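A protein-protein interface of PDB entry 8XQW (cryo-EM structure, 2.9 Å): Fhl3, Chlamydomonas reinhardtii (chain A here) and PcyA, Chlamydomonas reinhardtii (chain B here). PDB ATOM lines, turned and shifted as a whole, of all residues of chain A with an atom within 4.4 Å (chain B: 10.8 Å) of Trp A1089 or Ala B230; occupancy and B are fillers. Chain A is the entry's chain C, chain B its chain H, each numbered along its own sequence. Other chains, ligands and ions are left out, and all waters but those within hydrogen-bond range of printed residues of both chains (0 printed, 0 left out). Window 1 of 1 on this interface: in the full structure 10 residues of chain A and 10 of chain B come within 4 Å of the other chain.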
ATOM      1  N   TRP A1067       9.721  21.159   3.627  1.00  0.00           N
ATOM      2  CA  TRP A1067       9.057  21.714   4.799  1.00  0.00           C
ATOM      3  C   TRP A1067       7.665  21.145   5.004  1.00  0.00           C
ATOM      4  O   TRP A1067       7.308  20.773   6.127  1.00  0.00           O
ATOM      5  CB  TRP A1067       9.016  23.227   4.722  1.00  0.00           C
ATOM      6  CG  TRP A1067      10.114  23.813   5.488  1.00  0.00           C
ATOM      7  CD1 TRP A1067      11.311  24.183   5.011  1.00  0.00           C
ATOM      8  CD2 TRP A1067      10.135  24.083   6.882  1.00  0.00           C
ATOM      9  NE1 TRP A1067      12.091  24.677   6.015  1.00  0.00           N
ATOM     10  CE2 TRP A1067      11.382  24.629   7.179  1.00  0.00           C
ATOM     11  CE3 TRP A1067       9.214  23.921   7.909  1.00  0.00           C
ATOM     12  CZ2 TRP A1067      11.738  25.008   8.454  1.00  0.00           C
ATOM     13  CZ3 TRP A1067       9.568  24.305   9.170  1.00  0.00           C
ATOM     14  CH2 TRP A1067      10.815  24.844   9.433  1.00  0.00           C
ATOM     15  N   PHE A1068       6.862  21.060   3.966  1.00  0.00           N
ATOM     16  CA  PHE A1068       5.556  20.466   4.206  1.00  0.00           C
ATOM     17  C   PHE A1068       5.325  19.184   3.429  1.00  0.00           C
ATOM     18  O   PHE A1068       4.678  18.277   3.945  1.00  0.00           O
ATOM     19  CB  PHE A1068       4.465  21.486   3.929  1.00  0.00           C
ATOM     20  CG  PHE A1068       4.385  22.543   4.980  1.00  0.00           C
ATOM     21  CD1 PHE A1068       3.804  22.283   6.193  1.00  0.00           C
ATOM     22  CD2 PHE A1068       4.937  23.778   4.777  1.00  0.00           C
ATOM     23  CE1 PHE A1068       3.749  23.243   7.164  1.00  0.00           C
ATOM     24  CE2 PHE A1068       4.882  24.737   5.751  1.00  0.00           C
ATOM     25  CZ  PHE A1068       4.288  24.468   6.942  1.00  0.00           C
ATOM     26  N   ASP A1074       2.281  22.706   0.419  1.00  0.00           N
ATOM     27  CA  ASP A1074       3.555  22.529  -0.254  1.00  0.00           C
ATOM     28  C   ASP A1074       3.614  23.389  -1.506  1.00  0.00           C
ATOM     29  O   ASP A1074       2.597  23.701  -2.124  1.00  0.00           O
ATOM     30  CB  ASP A1074       3.769  21.062  -0.613  1.00  0.00           C
ATOM     31  CG  ASP A1074       5.150  20.791  -1.142  1.00  0.00           C
ATOM     32  OD1 ASP A1074       6.100  21.452  -0.688  1.00  0.00           O
ATOM     33  OD2 ASP A1074       5.288  19.915  -2.017  1.00  0.00           O
ATOM     34  N   PHE A1083      11.306  22.120  -7.200  1.00  0.00           N
ATOM     35  CA  PHE A1083      10.299  23.160  -7.141  1.00  0.00           C
ATOM     36  C   PHE A1083      10.202  23.846  -8.497  1.00  0.00           C
ATOM     37  O   PHE A1083      10.929  23.524  -9.434  1.00  0.00           O
ATOM     38  CB  PHE A1083      10.621  24.131  -6.020  1.00  0.00           C
ATOM     39  CG  PHE A1083      10.602  23.504  -4.670  1.00  0.00           C
ATOM     40  CD1 PHE A1083       9.421  23.104  -4.103  1.00  0.00           C
ATOM     41  CD2 PHE A1083      11.764  23.317  -3.967  1.00  0.00           C
ATOM     42  CE1 PHE A1083       9.401  22.535  -2.868  1.00  0.00           C
ATOM     43  CE2 PHE A1083      11.744  22.748  -2.728  1.00  0.00           C
ATOM     44  CZ  PHE A1083      10.562  22.356  -2.181  1.00  0.00           C
ATOM     45  N   TRP A1087      12.926  27.410  -7.270  1.00  0.00           N
ATOM     46  CA  TRP A1087      12.687  28.057  -5.998  1.00  0.00           C
ATOM     47  C   TRP A1087      13.220  27.201  -4.857  1.00  0.00           C
ATOM     48  O   TRP A1087      13.421  25.998  -4.993  1.00  0.00           O
ATOM     49  CB  TRP A1087      11.193  28.306  -5.844  1.00  0.00           C
ATOM     50  CG  TRP A1087      10.795  29.188  -4.745  1.00  0.00           C
ATOM     51  CD1 TRP A1087      10.926  30.531  -4.689  1.00  0.00           C
ATOM     52  CD2 TRP A1087      10.148  28.798  -3.545  1.00  0.00           C
ATOM     53  NE1 TRP A1087      10.423  31.005  -3.513  1.00  0.00           N
ATOM     54  CE2 TRP A1087       9.935  29.953  -2.792  1.00  0.00           C
ATOM     55  CE3 TRP A1087       9.737  27.575  -3.026  1.00  0.00           C
ATOM     56  CZ2 TRP A1087       9.337  29.923  -1.555  1.00  0.00           C
ATOM     57  CZ3 TRP A1087       9.144  27.549  -1.809  1.00  0.00           C
ATOM     58  CH2 TRP A1087       8.944  28.713  -1.084  1.00  0.00           C
ATOM     59  N   HIS A1088      13.466  27.843  -3.721  1.00  0.00           N
ATOM     60  CA  HIS A1088      13.927  27.180  -2.513  1.00  0.00           C
ATOM     61  C   HIS A1088      13.436  27.999  -1.340  1.00  0.00           C
ATOM     62  O   HIS A1088      13.327  29.218  -1.440  1.00  0.00           O
ATOM     63  CB  HIS A1088      15.448  27.069  -2.459  1.00  0.00           C
ATOM     64  CG  HIS A1088      16.010  25.962  -3.290  1.00  0.00           C
ATOM     65  ND1 HIS A1088      15.962  24.642  -2.905  1.00  0.00           N
ATOM     66  CD2 HIS A1088      16.656  25.983  -4.476  1.00  0.00           C
ATOM     67  CE1 HIS A1088      16.538  23.897  -3.827  1.00  0.00           C
ATOM     68  NE2 HIS A1088      16.968  24.686  -4.792  1.00  0.00           N
ATOM     69  N   TRP A1089      13.170  27.345  -0.215  1.00  0.00           N
ATOM     70  CA  TRP A1089      12.553  28.055   0.899  1.00  0.00           C
ATOM     71  C   TRP A1089      13.448  29.149   1.448  1.00  0.00           C
ATOM     72  O   TRP A1089      13.096  29.790   2.438  1.00  0.00           O
ATOM     73  CB  TRP A1089      12.183  27.082   2.005  1.00  0.00           C
ATOM     74  CG  TRP A1089      11.122  26.128   1.607  1.00  0.00           C
ATOM     75  CD1 TRP A1089      11.279  25.012   0.864  1.00  0.00           C
ATOM     76  CD2 TRP A1089       9.739  26.201   1.934  1.00  0.00           C
ATOM     77  NE1 TRP A1089      10.082  24.383   0.698  1.00  0.00           N
ATOM     78  CE2 TRP A1089       9.117  25.099   1.350  1.00  0.00           C
ATOM     79  CE3 TRP A1089       8.963  27.099   2.660  1.00  0.00           C
ATOM     80  CZ2 TRP A1089       7.764  24.869   1.469  1.00  0.00           C
ATOM     81  CZ3 TRP A1089       7.629  26.860   2.780  1.00  0.00           C
ATOM     82  CH2 TRP A1089       7.041  25.760   2.189  1.00  0.00           C
ATOM     83  N   ASN A1090      14.597  29.372   0.826  1.00  0.00           N
ATOM     84  CA  ASN A1090      15.511  30.422   1.244  1.00  0.00           C
ATOM     85  C   ASN A1090      15.182  31.755   0.594  1.00  0.00           C
ATOM     86  O   ASN A1090      15.322  32.801   1.229  1.00  0.00           O
ATOM     87  CB  ASN A1090      16.928  30.009   0.885  1.00  0.00           C
ATOM     88  CG  ASN A1090      17.888  30.280   1.975  1.00  0.00           C
ATOM     89  OD1 ASN A1090      17.493  30.536   3.106  1.00  0.00           O
ATOM     90  ND2 ASN A1090      19.168  30.232   1.657  1.00  0.00           N
ATOM     91  N   MET A1091      14.744  31.733  -0.667  1.00  0.00           N
ATOM     92  CA  MET A1091      14.581  32.927  -1.467  1.00  0.00           C
ATOM     93  C   MET A1091      13.677  33.933  -0.770  1.00  0.00           C
ATOM     94  O   MET A1091      12.808  33.555   0.010  1.00  0.00           O
ATOM     95  CB  MET A1091      14.003  32.562  -2.823  1.00  0.00           C
ATOM     96  CG  MET A1091      14.722  31.443  -3.505  1.00  0.00           C
ATOM     97  SD  MET A1091      16.479  31.723  -3.683  1.00  0.00           S
ATOM     98  CE  MET A1091      16.921  30.316  -4.678  1.00  0.00           C
ATOM     99  N   ARG B 171      27.646  30.279   5.118  1.00  0.00           N
ATOM    100  CA  ARG B 171      26.236  29.978   4.944  1.00  0.00           C
ATOM    101  C   ARG B 171      25.611  29.404   6.197  1.00  0.00           C
ATOM    102  O   ARG B 171      24.385  29.371   6.299  1.00  0.00           O
ATOM    103  CB  ARG B 171      26.045  29.024   3.779  1.00  0.00           C
ATOM    104  CG  ARG B 171      26.012  29.734   2.465  1.00  0.00           C
ATOM    105  CD  ARG B 171      26.493  28.842   1.370  1.00  0.00           C
ATOM    106  NE  ARG B 171      27.814  28.320   1.663  1.00  0.00           N
ATOM    107  CZ  ARG B 171      28.508  27.555   0.833  1.00  0.00           C
ATOM    108  NH1 ARG B 171      28.010  27.225  -0.343  1.00  0.00           N
ATOM    109  NH2 ARG B 171      29.702  27.121   1.188  1.00  0.00           N
ATOM    110  N   LEU B 172      26.415  28.961   7.155  1.00  0.00           N
ATOM    111  CA  LEU B 172      25.903  28.367   8.376  1.00  0.00           C
ATOM    112  C   LEU B 172      25.984  29.305   9.562  1.00  0.00           C
ATOM    113  O   LEU B 172      25.757  28.874  10.692  1.00  0.00           O
ATOM    114  CB  LEU B 172      26.641  27.074   8.692  1.00  0.00           C
ATOM    115  CG  LEU B 172      26.086  25.827   8.027  1.00  0.00           C
ATOM    116  CD1 LEU B 172      26.472  24.642   8.845  1.00  0.00           C
ATOM    117  CD2 LEU B 172      24.596  25.923   7.911  1.00  0.00           C
ATOM    118  N   LYS B 173      26.293  30.575   9.343  1.00  0.00           N
ATOM    119  CA  LYS B 173      26.123  31.523  10.426  1.00  0.00           C
ATOM    120  C   LYS B 173      24.645  31.593  10.782  1.00  0.00           C
ATOM    121  O   LYS B 173      23.801  30.971  10.137  1.00  0.00           O
ATOM    122  CB  LYS B 173      26.677  32.889  10.045  1.00  0.00           C
ATOM    123  CG  LYS B 173      25.947  33.585   8.930  1.00  0.00           C
ATOM    124  CD  LYS B 173      26.563  34.947   8.677  1.00  0.00           C
ATOM    125  CE  LYS B 173      25.811  35.723   7.626  1.00  0.00           C
ATOM    126  NZ  LYS B 173      25.348  34.872   6.510  1.00  0.00           N
ATOM    127  N   ASP B 174      24.342  32.349  11.837  1.00  0.00           N
ATOM    128  CA  ASP B 174      23.019  32.415  12.457  1.00  0.00           C
ATOM    129  C   ASP B 174      22.765  31.171  13.295  1.00  0.00           C
ATOM    130  O   ASP B 174      21.787  31.110  14.039  1.00  0.00           O
ATOM    131  CB  ASP B 174      21.907  32.564  11.415  1.00  0.00           C
ATOM    132  CG  ASP B 174      21.904  33.920  10.753  1.00  0.00           C
ATOM    133  OD1 ASP B 174      22.556  34.837  11.283  1.00  0.00           O
ATOM    134  OD2 ASP B 174      21.271  34.063   9.686  1.00  0.00           O
ATOM    135  N   ASP B 175      23.643  30.178  13.195  1.00  0.00           N
ATOM    136  CA  ASP B 175      23.548  28.961  13.986  1.00  0.00           C
ATOM    137  C   ASP B 175      24.754  28.754  14.877  1.00  0.00           C
ATOM    138  O   ASP B 175      24.798  27.778  15.625  1.00  0.00           O
ATOM    139  CB  ASP B 175      23.398  27.741  13.078  1.00  0.00           C
ATOM    140  CG  ASP B 175      22.254  27.873  12.117  1.00  0.00           C
ATOM    141  OD1 ASP B 175      21.342  28.676  12.390  1.00  0.00           O
ATOM    142  OD2 ASP B 175      22.264  27.174  11.084  1.00  0.00           O
ATOM    143  N   LEU B 214      29.919  22.120   1.993  1.00  0.00           N
ATOM    144  CA  LEU B 214      28.763  22.248   2.874  1.00  0.00           C
ATOM    145  C   LEU B 214      28.100  20.877   2.876  1.00  0.00           C
ATOM    146  O   LEU B 214      27.577  20.445   1.848  1.00  0.00           O
ATOM    147  CB  LEU B 214      27.818  23.329   2.391  1.00  0.00           C
ATOM    148  CG  LEU B 214      26.559  23.618   3.194  1.00  0.00           C
ATOM    149  CD1 LEU B 214      26.873  23.725   4.652  1.00  0.00           C
ATOM    150  CD2 LEU B 214      25.951  24.903   2.710  1.00  0.00           C
ATOM    151  N   VAL B 215      28.149  20.201   4.012  1.00  0.00           N
ATOM    152  CA  VAL B 215      27.747  18.807   4.114  1.00  0.00           C
ATOM    153  C   VAL B 215      26.606  18.699   5.106  1.00  0.00           C
ATOM    154  O   VAL B 215      26.675  19.264   6.201  1.00  0.00           O
ATOM    155  CB  VAL B 215      28.929  17.921   4.532  1.00  0.00           C
ATOM    156  CG1 VAL B 215      28.442  16.704   5.268  1.00  0.00           C
ATOM    157  CG2 VAL B 215      29.715  17.521   3.318  1.00  0.00           C
ATOM    158  N   ASP B 216      25.560  17.977   4.725  1.00  0.00           N
ATOM    159  CA  ASP B 216      24.373  17.804   5.545  1.00  0.00           C
ATOM    160  C   ASP B 216      24.036  16.327   5.641  1.00  0.00           C
ATOM    161  O   ASP B 216      24.102  15.605   4.647  1.00  0.00           O
ATOM    162  CB  ASP B 216      23.197  18.569   4.959  1.00  0.00           C
ATOM    163  CG  ASP B 216      22.008  18.593   5.877  1.00  0.00           C
ATOM    164  OD1 ASP B 216      22.134  18.131   7.023  1.00  0.00           O
ATOM    165  OD2 ASP B 216      20.941  19.075   5.456  1.00  0.00           O
ATOM    166  N   SER B 217      23.674  15.881   6.839  1.00  0.00           N
ATOM    167  CA  SER B 217      23.390  14.468   7.041  1.00  0.00           C
ATOM    168  C   SER B 217      22.034  14.058   6.496  1.00  0.00           C
ATOM    169  O   SER B 217      21.877  12.911   6.071  1.00  0.00           O
ATOM    170  CB  SER B 217      23.469  14.120   8.523  1.00  0.00           C
ATOM    171  OG  SER B 217      22.179  14.020   9.083  1.00  0.00           O
ATOM    172  N   MET B 218      21.057  14.961   6.491  1.00  0.00           N
ATOM    173  CA  MET B 218      19.737  14.653   5.962  1.00  0.00           C
ATOM    174  C   MET B 218      19.684  14.693   4.446  1.00  0.00           C
ATOM    175  O   MET B 218      18.596  14.575   3.884  1.00  0.00           O
ATOM    176  CB  MET B 218      18.703  15.626   6.516  1.00  0.00           C
ATOM    177  CG  MET B 218      18.719  15.760   8.014  1.00  0.00           C
ATOM    178  SD  MET B 218      17.589  14.622   8.809  1.00  0.00           S
ATOM    179  CE  MET B 218      16.078  15.034   7.963  1.00  0.00           C
ATOM    180  N   ASP B 219      20.822  14.859   3.776  1.00  0.00           N
ATOM    181  CA  ASP B 219      20.866  14.940   2.316  1.00  0.00           C
ATOM    182  C   ASP B 219      22.269  14.590   1.845  1.00  0.00           C
ATOM    183  O   ASP B 219      23.016  15.444   1.363  1.00  0.00           O
ATOM    184  CB  ASP B 219      20.457  16.334   1.849  1.00  0.00           C
ATOM    185  CG  ASP B 219      20.454  16.470   0.352  1.00  0.00           C
ATOM    186  OD1 ASP B 219      20.415  15.434  -0.336  1.00  0.00           O
ATOM    187  OD2 ASP B 219      20.495  17.615  -0.136  1.00  0.00           O
ATOM    188  N   LEU B 224      19.251  18.493  -3.335  1.00  0.00           N
ATOM    189  CA  LEU B 224      18.706  19.827  -3.150  1.00  0.00           C
ATOM    190  C   LEU B 224      19.732  20.898  -3.471  1.00  0.00           C
ATOM    191  O   LEU B 224      19.525  22.061  -3.126  1.00  0.00           O
ATOM    192  CB  LEU B 224      18.185  19.996  -1.727  1.00  0.00           C
ATOM    193  CG  LEU B 224      16.942  19.168  -1.456  1.00  0.00           C
ATOM    194  CD1 LEU B 224      16.599  19.201   0.004  1.00  0.00           C
ATOM    195  CD2 LEU B 224      15.805  19.704  -2.270  1.00  0.00           C
ATOM    196  N   GLU B 225      20.844  20.523  -4.098  1.00  0.00           N
ATOM    197  CA  GLU B 225      21.842  21.451  -4.618  1.00  0.00           C
ATOM    198  C   GLU B 225      22.480  22.298  -3.536  1.00  0.00           C
ATOM    199  O   GLU B 225      22.896  23.425  -3.795  1.00  0.00           O
ATOM    200  CB  GLU B 225      21.243  22.355  -5.689  1.00  0.00           C
ATOM    201  CG  GLU B 225      20.863  21.627  -6.943  1.00  0.00           C
ATOM    202  CD  GLU B 225      19.661  22.238  -7.607  1.00  0.00           C
ATOM    203  OE1 GLU B 225      18.580  21.612  -7.574  1.00  0.00           O
ATOM    204  OE2 GLU B 225      19.791  23.353  -8.152  1.00  0.00           O
ATOM    205  N   GLY B 226      22.576  21.792  -2.320  1.00  0.00           N
ATOM    206  CA  GLY B 226      23.237  22.532  -1.277  1.00  0.00           C
ATOM    207  C   GLY B 226      22.381  23.538  -0.559  1.00  0.00           C
ATOM    208  O   GLY B 226      22.924  24.386   0.151  1.00  0.00           O
ATOM    209  N   PHE B 227      21.065  23.488  -0.726  1.00  0.00           N
ATOM    210  CA  PHE B 227      20.163  24.300   0.070  1.00  0.00           C
ATOM    211  C   PHE B 227      19.483  23.496   1.161  1.00  0.00           C
ATOM    212  O   PHE B 227      18.513  23.969   1.752  1.00  0.00           O
ATOM    213  CB  PHE B 227      19.117  24.960  -0.813  1.00  0.00           C
ATOM    214  CG  PHE B 227      19.671  25.988  -1.740  1.00  0.00           C
ATOM    215  CD1 PHE B 227      20.203  25.623  -2.948  1.00  0.00           C
ATOM    216  CD2 PHE B 227      19.634  27.321  -1.416  1.00  0.00           C
ATOM    217  CE1 PHE B 227      20.699  26.560  -3.801  1.00  0.00           C
ATOM    218  CE2 PHE B 227      20.129  28.259  -2.276  1.00  0.00           C
ATOM    219  CZ  PHE B 227      20.659  27.877  -3.467  1.00  0.00           C
ATOM    220  N   SER B 228      19.982  22.298   1.451  1.00  0.00           N
ATOM    221  CA  SER B 228      19.384  21.466   2.478  1.00  0.00           C
ATOM    222  C   SER B 228      19.412  22.117   3.846  1.00  0.00           C
ATOM    223  O   SER B 228      18.637  21.725   4.718  1.00  0.00           O
ATOM    224  CB  SER B 228      20.105  20.131   2.545  1.00  0.00           C
ATOM    225  OG  SER B 228      20.045  19.463   1.303  1.00  0.00           O
ATOM    226  N   TYR B 229      20.292  23.080   4.074  1.00  0.00           N
ATOM    227  CA  TYR B 229      20.257  23.768   5.353  1.00  0.00           C
ATOM    228  C   TYR B 229      19.037  24.658   5.488  1.00  0.00           C
ATOM    229  O   TYR B 229      18.791  25.179   6.577  1.00  0.00           O
ATOM    230  CB  TYR B 229      21.525  24.593   5.549  1.00  0.00           C
ATOM    231  CG  TYR B 229      21.606  25.786   4.644  1.00  0.00           C
ATOM    232  CD1 TYR B 229      22.014  25.652   3.339  1.00  0.00           C
ATOM    233  CD2 TYR B 229      21.267  27.040   5.094  1.00  0.00           C
ATOM    234  CE1 TYR B 229      22.077  26.727   2.513  1.00  0.00           C
ATOM    235  CE2 TYR B 229      21.330  28.121   4.274  1.00  0.00           C
ATOM    236  CZ  TYR B 229      21.731  27.960   2.986  1.00  0.00           C
ATOM    237  OH  TYR B 229      21.794  29.048   2.162  1.00  0.00           O
ATOM    238  N   ALA B 230      18.274  24.843   4.415  1.00  0.00           N
ATOM    239  CA  ALA B 230      17.111  25.711   4.436  1.00  0.00           C
ATOM    240  C   ALA B 230      15.824  25.033   4.019  1.00  0.00           C
ATOM    241  O   ALA B 230      14.756  25.483   4.438  1.00  0.00           O
ATOM    242  CB  ALA B 230      17.328  26.924   3.527  1.00  0.00           C
ATOM    243  N   ASP B 231      15.880  23.968   3.228  1.00  0.00           N
ATOM    244  CA  ASP B 231      14.685  23.302   2.749  1.00  0.00           C
ATOM    245  C   ASP B 231      14.131  22.272   3.714  1.00  0.00           C
ATOM    246  O   ASP B 231      12.920  22.055   3.720  1.00  0.00           O
ATOM    247  CB  ASP B 231      14.967  22.605   1.420  1.00  0.00           C
ATOM    248  CG  ASP B 231      14.838  23.527   0.246  1.00  0.00           C
ATOM    249  OD1 ASP B 231      14.343  24.649   0.435  1.00  0.00           O
ATOM    250  OD2 ASP B 231      15.227  23.142  -0.872  1.00  0.00           O
ATOM    251  N   ILE B 232      14.969  21.632   4.515  1.00  0.00           N
ATOM    252  CA  ILE B 232      14.580  20.476   5.306  1.00  0.00           C
ATOM    253  C   ILE B 232      14.522  20.887   6.769  1.00  0.00           C
ATOM    254  O   ILE B 232      15.525  21.336   7.322  1.00  0.00           O
ATOM    255  CB  ILE B 232      15.560  19.309   5.112  1.00  0.00           C
ATOM    256  CG1 ILE B 232      15.712  19.018   3.629  1.00  0.00           C
ATOM    257  CG2 ILE B 232      15.076  18.100   5.832  1.00  0.00           C
ATOM    258  CD1 ILE B 232      16.491  17.801   3.343  1.00  0.00           C
ATOM    259  N   PRO B 233      13.387  20.752   7.440  1.00  0.00           N
ATOM    260  CA  PRO B 233      13.309  21.145   8.844  1.00  0.00           C
ATOM    261  C   PRO B 233      14.000  20.123   9.726  1.00  0.00           C
ATOM    262  O   PRO B 233      14.274  18.995   9.326  1.00  0.00           O
ATOM    263  CB  PRO B 233      11.809  21.189   9.101  1.00  0.00           C
ATOM    264  CG  PRO B 233      11.276  20.184   8.196  1.00  0.00           C
ATOM    265  CD  PRO B 233      12.119  20.186   6.970  1.00  0.00           C
ATOM    266  N   ASP B 234      14.285  20.538  10.950  1.00  0.00           N
ATOM    267  CA  ASP B 234      15.032  19.678  11.848  1.00  0.00           C
ATOM    268  C   ASP B 234      14.176  18.493  12.281  1.00  0.00           C
ATOM    269  O   ASP B 234      13.022  18.673  12.674  1.00  0.00           O
ATOM    270  CB  ASP B 234      15.492  20.456  13.074  1.00  0.00           C
ATOM    271  CG  ASP B 234      16.752  21.245  12.819  1.00  0.00           C
ATOM    272  OD1 ASP B 234      17.337  21.094  11.727  1.00  0.00           O
ATOM    273  OD2 ASP B 234      17.162  22.018  13.708  1.00  0.00           O
ATOM    274  N   ARG B 244      20.790  15.740  13.624  1.00  0.00           N
ATOM    275  CA  ARG B 244      21.295  16.164  12.299  1.00  0.00           C
ATOM    276  C   ARG B 244      22.709  16.716  12.442  1.00  0.00           C
ATOM    277  O   ARG B 244      23.007  17.293  13.479  1.00  0.00           O
ATOM    278  CB  ARG B 244      20.339  17.200  11.718  1.00  0.00           C
ATOM    279  CG  ARG B 244      20.653  17.742  10.335  1.00  0.00           C
ATOM    280  CD  ARG B 244      19.969  19.077  10.177  1.00  0.00           C
ATOM    281  NE  ARG B 244      19.367  19.188   8.849  1.00  0.00           N
ATOM    282  CZ  ARG B 244      18.694  20.240   8.440  1.00  0.00           C
ATOM    283  NH1 ARG B 244      18.321  21.157   9.304  1.00  0.00           N
ATOM    284  NH2 ARG B 244      18.407  20.375   7.165  1.00  0.00           N
ATOM    285  N   GLN B 246      25.785  19.038  10.450  1.00  0.00           N
ATOM    286  CA  GLN B 246      26.121  19.969   9.385  1.00  0.00           C
ATOM    287  C   GLN B 246      27.582  20.361   9.489  1.00  0.00           C
ATOM    288  O   GLN B 246      28.085  20.609  10.581  1.00  0.00           O
ATOM    289  CB  GLN B 246      25.275  21.218   9.454  1.00  0.00           C
ATOM    290  CG  GLN B 246      23.848  20.962   9.769  1.00  0.00           C
ATOM    291  CD  GLN B 246      22.950  21.889   9.026  1.00  0.00           C
ATOM    292  OE1 GLN B 246      22.468  22.874   9.569  1.00  0.00           O
ATOM    293  NE2 GLN B 246      22.719  21.586   7.764  1.00  0.00           N
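The backbone NH (N) of Trp A1089 lies within hydrogen-bond range of the side-chain carboxylate (OD1) of Asp B231 (3.0 Å).
The backbone NH (N) of Trp A1067 lies close to the backbone carbonyl oxygen (O) of Asp B231, at 3.3 Å.
A ring nitrogen (ND1) of His A1088 lies within hydrogen-bond range of the side-chain carboxylate (OD2) of Asp B231.
O of Ala B230 sits at hydrogen-bond distance from NE1 of Trp A1067 (3.2 Å).
The side-chain amide nitrogen (ND2) of Asn A1090 lies within hydrogen-bond range of the side-chain hydroxyl (OH) of Tyr B229, 2.9 Å away.
Among the printed residues, pairs that only touch across the chains: Trp A1067 with Pro B233, Phe A1083 with Asp B231, His A1088 with Leu B224, His A1088 with Phe B227, Trp A1089 with Ala B230 and Asn A1090 with Ala B230.
Of the printed residues of chain B, Trp A1067 touches Ala B230 (3.2 Å), Asp B231 (3.0 Å) and Pro B233 (3.8 Å).
Asp A1074 touches none of the printed residues of chain B.
Of the printed residues of chain B, Phe A1083 touches Asp B231 (3.97 Å).
Of chain B, only Leu B224 (3.6 Å), Phe B227 (3.8 Å) and Asp B231 (2.6 Å) come within 4 Å of His A1088.
Asn A1090 touches two residues of chain B.
No residue of chain B comes within 4 Å of Met A1091.
Of the printed residues of chain A, Leu B224 touches His A1088.
Of the printed residues of chain A, Phe B227 touches His A1088 (3.8 Å).
Of the printed residues of chain A, Asp B231 touches Trp A1067 (3.0 Å), Phe A1083 (3.97 Å), His A1088 (2.6 Å) and Trp A1089 (3.0 Å).
Asp B234 touches none of the printed residues of chain A.
The nearest residue of chain B that does not touch Trp A1089 is Ile B232 (6.2 Å).
Of the 24 printed residues of chain B, 6 touch a printed residue of chain A.
Printed residues of chain B that touch a printed residue of chain A: Leu B224, Phe B227, Tyr B229, Ala B230, Asp B231 and Pro B233.
Hydrophobic or aromatic side chains of chain B within 4 Å of the printed part of chain A: Phe B227, Tyr B229, Ala B230 and Pro B233.
Among the printed residues, 11 pairs touch across the chains.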
